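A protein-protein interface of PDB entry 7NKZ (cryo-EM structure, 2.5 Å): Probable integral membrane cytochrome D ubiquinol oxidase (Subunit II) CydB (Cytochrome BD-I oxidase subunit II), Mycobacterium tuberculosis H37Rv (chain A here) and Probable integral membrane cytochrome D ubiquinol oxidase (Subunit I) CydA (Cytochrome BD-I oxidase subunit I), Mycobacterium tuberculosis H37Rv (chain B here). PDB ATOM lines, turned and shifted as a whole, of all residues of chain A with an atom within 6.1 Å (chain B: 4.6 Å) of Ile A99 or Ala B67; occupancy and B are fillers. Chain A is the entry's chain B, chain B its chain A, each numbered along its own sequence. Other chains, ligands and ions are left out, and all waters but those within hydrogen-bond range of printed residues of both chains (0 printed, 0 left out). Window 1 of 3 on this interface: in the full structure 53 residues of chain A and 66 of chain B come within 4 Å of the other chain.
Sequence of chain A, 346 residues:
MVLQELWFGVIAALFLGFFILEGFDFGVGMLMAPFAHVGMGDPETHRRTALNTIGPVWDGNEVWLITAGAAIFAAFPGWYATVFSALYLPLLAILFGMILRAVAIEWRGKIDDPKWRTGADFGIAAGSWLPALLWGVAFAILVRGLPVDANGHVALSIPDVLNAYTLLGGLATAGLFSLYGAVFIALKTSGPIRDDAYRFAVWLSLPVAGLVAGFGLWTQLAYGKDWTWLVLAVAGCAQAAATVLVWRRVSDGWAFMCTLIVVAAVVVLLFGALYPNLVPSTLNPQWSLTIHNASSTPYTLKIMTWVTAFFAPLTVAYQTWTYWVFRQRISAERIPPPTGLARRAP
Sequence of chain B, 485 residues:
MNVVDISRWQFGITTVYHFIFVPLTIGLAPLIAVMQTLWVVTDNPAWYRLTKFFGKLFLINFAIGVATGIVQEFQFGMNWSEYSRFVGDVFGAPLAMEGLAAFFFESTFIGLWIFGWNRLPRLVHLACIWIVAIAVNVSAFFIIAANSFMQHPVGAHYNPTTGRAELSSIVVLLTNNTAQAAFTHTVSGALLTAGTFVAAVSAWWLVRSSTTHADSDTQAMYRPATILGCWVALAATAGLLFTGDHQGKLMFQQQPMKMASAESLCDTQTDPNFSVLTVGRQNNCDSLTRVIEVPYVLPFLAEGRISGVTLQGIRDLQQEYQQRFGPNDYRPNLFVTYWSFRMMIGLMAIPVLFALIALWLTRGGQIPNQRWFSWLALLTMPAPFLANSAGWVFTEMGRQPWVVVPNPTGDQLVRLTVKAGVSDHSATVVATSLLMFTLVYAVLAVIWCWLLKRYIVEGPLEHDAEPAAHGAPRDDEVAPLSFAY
O of Ile B64 lies within hydrogen-bond range of OG1 of Thr B68, at 3.0 Å.
Among the printed residues, merely in contact across the chains: Met A98 with Ile B70 (3.3 Å), Ile A99 with Tyr B441 (3.3 Å), Ile A99 with Ala B67 (3.5 Å), Ala A102 with Ala B63 (3.5 Å), Phe A96 with Val B440 (3.5 Å), Ile A99 with Val B71 (3.6 Å), Val A103 with Ile B64 (3.6 Å), Ala A102 with Ala B67 (3.6 Å), Val A103 with Ala B67 (3.7 Å), Ile A99 with Leu B444 (3.7 Å), Leu A95 with Val B71 (3.8 Å), Val A103 with Ala B63 (3.8 Å), Val A103 with Leu B444 (3.8 Å) and Leu A95 with Ile B70 (3.9 Å).
Ile A99 touches just these residues of chain B: Ala B67, Val B71, Tyr B441 and Leu B444. Leu A100 touches none of the printed residues of chain B. Of the printed residues of chain B, Val A103 touches Ala B63 (3.8 Å), Ile B64 (3.6 Å), Ala B67 (3.7 Å) and Leu B444 (3.8 Å). Printed residues of chain A within 4 Å of Ile B70: Leu A95 and Met A98. Of the printed residues of chain A, Val B440 touches Phe A96. Printed residues of chain A within 4 Å of Tyr B441: Ile A99. The nearest residue of chain A that does not touch Ala B67 is Met A98 (5.2 Å).
Printed residues of chain A that touch a printed residue of chain B: Leu A95, Phe A96, Met A98, Ile A99, Ala A102 and Val A103. Printed residues of chain B that touch a printed residue of chain A: Ala B63, Ile B64, Ala B67, Ile B70, Val B71, Val B440, Tyr B441 and Leu B444. Among the printed residues, no Asp or Glu carboxylate lies within 4 Å of a Lys or Arg side-chain nitrogen of the other chain.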
ATOM      1  N   ILE A  94       3.800  -3.807 -25.898  1.00  0.00           N
ATOM      2  CA  ILE A  94       3.147  -2.544 -25.564  1.00  0.00           C
ATOM      3  C   ILE A  94       4.169  -1.550 -25.028  1.00  0.00           C
ATOM      4  O   ILE A  94       4.190  -0.376 -25.419  1.00  0.00           O
ATOM      5  CB  ILE A  94       2.006  -2.778 -24.556  1.00  0.00           C
ATOM      6  CG1 ILE A  94       0.853  -3.532 -25.218  1.00  0.00           C
ATOM      7  CG2 ILE A  94       1.517  -1.460 -23.981  1.00  0.00           C
ATOM      8  CD1 ILE A  94      -0.308  -3.810 -24.289  1.00  0.00           C
ATOM      9  N   LEU A  95       5.039  -2.010 -24.126  1.00  0.00           N
ATOM     10  CA  LEU A  95       6.084  -1.143 -23.595  1.00  0.00           C
ATOM     11  C   LEU A  95       7.105  -0.772 -24.660  1.00  0.00           C
ATOM     12  O   LEU A  95       7.628   0.347 -24.650  1.00  0.00           O
ATOM     13  CB  LEU A  95       6.776  -1.818 -22.410  1.00  0.00           C
ATOM     14  CG  LEU A  95       5.857  -2.213 -21.255  1.00  0.00           C
ATOM     15  CD1 LEU A  95       6.647  -2.862 -20.129  1.00  0.00           C
ATOM     16  CD2 LEU A  95       5.092  -1.000 -20.757  1.00  0.00           C
ATOM     17  N   PHE A  96       7.402  -1.693 -25.581  1.00  0.00           N
ATOM     18  CA  PHE A  96       8.369  -1.403 -26.635  1.00  0.00           C
ATOM     19  C   PHE A  96       7.914  -0.233 -27.497  1.00  0.00           C
ATOM     20  O   PHE A  96       8.707   0.663 -27.811  1.00  0.00           O
ATOM     21  CB  PHE A  96       8.593  -2.647 -27.494  1.00  0.00           C
ATOM     22  CG  PHE A  96       9.402  -2.391 -28.734  1.00  0.00           C
ATOM     23  CD1 PHE A  96      10.778  -2.258 -28.666  1.00  0.00           C
ATOM     24  CD2 PHE A  96       8.784  -2.288 -29.970  1.00  0.00           C
ATOM     25  CE1 PHE A  96      11.524  -2.023 -29.806  1.00  0.00           C
ATOM     26  CE2 PHE A  96       9.524  -2.053 -31.113  1.00  0.00           C
ATOM     27  CZ  PHE A  96      10.894  -1.921 -31.031  1.00  0.00           C
ATOM     28  N   GLY A  97       6.643  -0.221 -27.889  1.00  0.00           N
ATOM     29  CA  GLY A  97       6.114   0.859 -28.696  1.00  0.00           C
ATOM     30  C   GLY A  97       6.056   2.192 -27.978  1.00  0.00           C
ATOM     31  O   GLY A  97       6.451   3.219 -28.535  1.00  0.00           O
ATOM     32  N   MET A  98       5.537   2.161 -26.750  1.00  0.00           N
ATOM     33  CA  MET A  98       5.394   3.332 -25.884  1.00  0.00           C
ATOM     34  C   MET A  98       6.709   4.050 -25.666  1.00  0.00           C
ATOM     35  O   MET A  98       6.766   5.273 -25.664  1.00  0.00           O
ATOM     36  CB  MET A  98       4.864   2.920 -24.517  1.00  0.00           C
ATOM     37  CG  MET A  98       3.389   2.587 -24.467  1.00  0.00           C
ATOM     38  SD  MET A  98       2.941   2.052 -22.808  1.00  0.00           S
ATOM     39  CE  MET A  98       2.992   3.602 -21.919  1.00  0.00           C
ATOM     40  N   ILE A  99       7.760   3.276 -25.440  1.00  0.00           N
ATOM     41  CA  ILE A  99       9.090   3.842 -25.240  1.00  0.00           C
ATOM     42  C   ILE A  99       9.526   4.619 -26.475  1.00  0.00           C
ATOM     43  O   ILE A  99      10.044   5.737 -26.372  1.00  0.00           O
ATOM     44  CB  ILE A  99      10.100   2.734 -24.888  1.00  0.00           C
ATOM     45  CG1 ILE A  99       9.861   2.209 -23.474  1.00  0.00           C
ATOM     46  CG2 ILE A  99      11.527   3.244 -25.027  1.00  0.00           C
ATOM     47  CD1 ILE A  99      10.747   1.041 -23.119  1.00  0.00           C
ATOM     48  N   LEU A 100       9.323   4.040 -27.660  1.00  0.00           N
ATOM     49  CA  LEU A 100       9.706   4.715 -28.894  1.00  0.00           C
ATOM     50  C   LEU A 100       8.885   5.980 -29.115  1.00  0.00           C
ATOM     51  O   LEU A 100       9.428   7.015 -29.519  1.00  0.00           O
ATOM     52  CB  LEU A 100       9.558   3.763 -30.080  1.00  0.00           C
ATOM     53  CG  LEU A 100      10.429   2.506 -30.048  1.00  0.00           C
ATOM     54  CD1 LEU A 100      10.232   1.683 -31.312  1.00  0.00           C
ATOM     55  CD2 LEU A 100      11.894   2.871 -29.862  1.00  0.00           C
ATOM     56  N   ARG A 101       7.576   5.919 -28.854  1.00  0.00           N
ATOM     57  CA  ARG A 101       6.730   7.089 -29.066  1.00  0.00           C
ATOM     58  C   ARG A 101       7.051   8.203 -28.079  1.00  0.00           C
ATOM     59  O   ARG A 101       6.922   9.385 -28.420  1.00  0.00           O
ATOM     60  CB  ARG A 101       5.255   6.702 -28.963  1.00  0.00           C
ATOM     61  CG  ARG A 101       4.309   7.742 -29.541  1.00  0.00           C
ATOM     62  CD  ARG A 101       2.874   7.509 -29.099  1.00  0.00           C
ATOM     63  NE  ARG A 101       2.713   7.676 -27.658  1.00  0.00           N
ATOM     64  CZ  ARG A 101       1.541   7.837 -27.051  1.00  0.00           C
ATOM     65  NH1 ARG A 101       0.422   7.854 -27.762  1.00  0.00           N
ATOM     66  NH2 ARG A 101       1.487   7.981 -25.735  1.00  0.00           N
ATOM     67  N   ALA A 102       7.465   7.853 -26.859  1.00  0.00           N
ATOM     68  CA  ALA A 102       7.782   8.868 -25.861  1.00  0.00           C
ATOM     69  C   ALA A 102       9.006   9.691 -26.237  1.00  0.00           C
ATOM     70  O   ALA A 102       9.149  10.819 -25.753  1.00  0.00           O
ATOM     71  CB  ALA A 102       7.992   8.215 -24.495  1.00  0.00           C
ATOM     72  N   VAL A 103       9.885   9.160 -27.084  1.00  0.00           N
ATOM     73  CA  VAL A 103      11.062   9.895 -27.526  1.00  0.00           C
ATOM     74  C   VAL A 103      10.960  10.359 -28.973  1.00  0.00           C
ATOM     75  O   VAL A 103      11.612  11.354 -29.330  1.00  0.00           O
ATOM     76  CB  VAL A 103      12.348   9.065 -27.325  1.00  0.00           C
ATOM     77  CG1 VAL A 103      12.537   8.729 -25.857  1.00  0.00           C
ATOM     78  CG2 VAL A 103      12.304   7.797 -28.164  1.00  0.00           C
ATOM     79  N   ALA A 104      10.169   9.687 -29.813  1.00  0.00           N
ATOM     80  CA  ALA A 104      10.088  10.075 -31.218  1.00  0.00           C
ATOM     81  C   ALA A 104       9.323  11.378 -31.405  1.00  0.00           C
ATOM     82  O   ALA A 104       9.658  12.165 -32.297  1.00  0.00           O
ATOM     83  CB  ALA A 104       9.437   8.960 -32.036  1.00  0.00           C
ATOM     84  N   ALA B  63      12.098  13.864 -22.410  1.00  0.00           N
ATOM     85  CA  ALA B  63      11.390  12.886 -23.232  1.00  0.00           C
ATOM     86  C   ALA B  63      11.904  11.474 -22.983  1.00  0.00           C
ATOM     87  O   ALA B  63      11.117  10.532 -22.835  1.00  0.00           O
ATOM     88  CB  ALA B  63      11.519  13.253 -24.709  1.00  0.00           C
ATOM     89  N   ILE B  64      13.229  11.306 -22.935  1.00  0.00           N
ATOM     90  CA  ILE B  64      13.793   9.988 -22.680  1.00  0.00           C
ATOM     91  C   ILE B  64      13.669   9.604 -21.211  1.00  0.00           C
ATOM     92  O   ILE B  64      13.672   8.411 -20.884  1.00  0.00           O
ATOM     93  CB  ILE B  64      15.257   9.936 -23.159  1.00  0.00           C
ATOM     94  CG1 ILE B  64      15.748   8.487 -23.237  1.00  0.00           C
ATOM     95  CG2 ILE B  64      16.147  10.780 -22.267  1.00  0.00           C
ATOM     96  CD1 ILE B  64      17.048   8.321 -23.985  1.00  0.00           C
ATOM     97  N   GLY B  65      13.550  10.585 -20.314  1.00  0.00           N
ATOM     98  CA  GLY B  65      13.282  10.270 -18.922  1.00  0.00           C
ATOM     99  C   GLY B  65      11.914   9.654 -18.711  1.00  0.00           C
ATOM    100  O   GLY B  65      11.757   8.756 -17.880  1.00  0.00           O
ATOM    101  N   VAL B  66      10.911  10.125 -19.453  1.00  0.00           N
ATOM    102  CA  VAL B  66       9.582   9.527 -19.376  1.00  0.00           C
ATOM    103  C   VAL B  66       9.595   8.121 -19.963  1.00  0.00           C
ATOM    104  O   VAL B  66       8.991   7.197 -19.408  1.00  0.00           O
ATOM    105  CB  VAL B  66       8.552  10.426 -20.084  1.00  0.00           C
ATOM    106  CG1 VAL B  66       7.185   9.758 -20.107  1.00  0.00           C
ATOM    107  CG2 VAL B  66       8.475  11.783 -19.406  1.00  0.00           C
ATOM    108  N   ALA B  67      10.290   7.937 -21.089  1.00  0.00           N
ATOM    109  CA  ALA B  67      10.286   6.644 -21.768  1.00  0.00           C
ATOM    110  C   ALA B  67      10.902   5.553 -20.901  1.00  0.00           C
ATOM    111  O   ALA B  67      10.393   4.426 -20.855  1.00  0.00           O
ATOM    112  CB  ALA B  67      11.027   6.750 -23.099  1.00  0.00           C
ATOM    113  N   THR B  68      11.997   5.864 -20.209  1.00  0.00           N
ATOM    114  CA  THR B  68      12.680   4.873 -19.388  1.00  0.00           C
ATOM    115  C   THR B  68      11.941   4.555 -18.094  1.00  0.00           C
ATOM    116  O   THR B  68      12.299   3.582 -17.422  1.00  0.00           O
ATOM    117  CB  THR B  68      14.099   5.345 -19.062  1.00  0.00           C
ATOM    118  OG1 THR B  68      14.053   6.672 -18.525  1.00  0.00           O
ATOM    119  CG2 THR B  68      14.961   5.339 -20.315  1.00  0.00           C
ATOM    120  N   GLY B  69      10.933   5.341 -17.728  1.00  0.00           N
ATOM    121  CA  GLY B  69      10.177   5.077 -16.520  1.00  0.00           C
ATOM    122  C   GLY B  69       8.889   4.319 -16.764  1.00  0.00           C
ATOM    123  O   GLY B  69       8.248   3.853 -15.817  1.00  0.00           O
ATOM    124  N   ILE B  70       8.499   4.189 -18.033  1.00  0.00           N
ATOM    125  CA  ILE B  70       7.249   3.510 -18.367  1.00  0.00           C
ATOM    126  C   ILE B  70       7.321   2.034 -17.989  1.00  0.00           C
ATOM    127  O   ILE B  70       6.382   1.482 -17.402  1.00  0.00           O
ATOM    128  CB  ILE B  70       6.921   3.692 -19.859  1.00  0.00           C
ATOM    129  CG1 ILE B  70       6.683   5.168 -20.180  1.00  0.00           C
ATOM    130  CG2 ILE B  70       5.720   2.854 -20.239  1.00  0.00           C
ATOM    131  CD1 ILE B  70       6.549   5.459 -21.657  1.00  0.00           C
ATOM    132  N   VAL B  71       8.433   1.375 -18.322  1.00  0.00           N
ATOM    133  CA  VAL B  71       8.570  -0.050 -18.029  1.00  0.00           C
ATOM    134  C   VAL B  71       8.534  -0.293 -16.527  1.00  0.00           C
ATOM    135  O   VAL B  71       7.892  -1.237 -16.052  1.00  0.00           O
ATOM    136  CB  VAL B  71       9.859  -0.605 -18.663  1.00  0.00           C
ATOM    137  CG1 VAL B  71      10.171  -1.989 -18.116  1.00  0.00           C
ATOM    138  CG2 VAL B  71       9.717  -0.657 -20.168  1.00  0.00           C
ATOM    139  N   VAL B 440      17.408  -1.438 -26.936  1.00  0.00           N
ATOM    140  CA  VAL B 440      16.557  -0.282 -27.205  1.00  0.00           C
ATOM    141  C   VAL B 440      16.997   0.914 -26.370  1.00  0.00           C
ATOM    142  O   VAL B 440      17.110   2.036 -26.879  1.00  0.00           O
ATOM    143  CB  VAL B 440      15.079  -0.636 -26.959  1.00  0.00           C
ATOM    144  CG1 VAL B 440      14.231   0.624 -26.901  1.00  0.00           C
ATOM    145  CG2 VAL B 440      14.574  -1.563 -28.051  1.00  0.00           C
ATOM    146  N   TYR B 441      17.263   0.696 -25.080  1.00  0.00           N
ATOM    147  CA  TYR B 441      17.745   1.784 -24.236  1.00  0.00           C
ATOM    148  C   TYR B 441      19.144   2.234 -24.640  1.00  0.00           C
ATOM    149  O   TYR B 441      19.455   3.427 -24.557  1.00  0.00           O
ATOM    150  CB  TYR B 441      17.725   1.361 -22.769  1.00  0.00           C
ATOM    151  CG  TYR B 441      16.354   1.400 -22.136  1.00  0.00           C
ATOM    152  CD1 TYR B 441      15.337   2.171 -22.683  1.00  0.00           C
ATOM    153  CD2 TYR B 441      16.076   0.670 -20.988  1.00  0.00           C
ATOM    154  CE1 TYR B 441      14.081   2.210 -22.107  1.00  0.00           C
ATOM    155  CE2 TYR B 441      14.824   0.703 -20.405  1.00  0.00           C
ATOM    156  CZ  TYR B 441      13.831   1.475 -20.968  1.00  0.00           C
ATOM    157  OH  TYR B 441      12.583   1.511 -20.391  1.00  0.00           O
ATOM    158  N   LEU B 444      18.808   4.516 -27.672  1.00  0.00           N
ATOM    159  CA  LEU B 444      18.266   5.806 -27.262  1.00  0.00           C
ATOM    160  C   LEU B 444      19.270   6.604 -26.439  1.00  0.00           C
ATOM    161  O   LEU B 444      19.316   7.835 -26.548  1.00  0.00           O
ATOM    162  CB  LEU B 444      16.971   5.608 -26.475  1.00  0.00           C
ATOM    163  CG  LEU B 444      15.797   5.001 -27.246  1.00  0.00           C
ATOM    164  CD1 LEU B 444      14.558   4.932 -26.370  1.00  0.00           C
ATOM    165  CD2 LEU B 444      15.519   5.791 -28.516  1.00  0.00           C
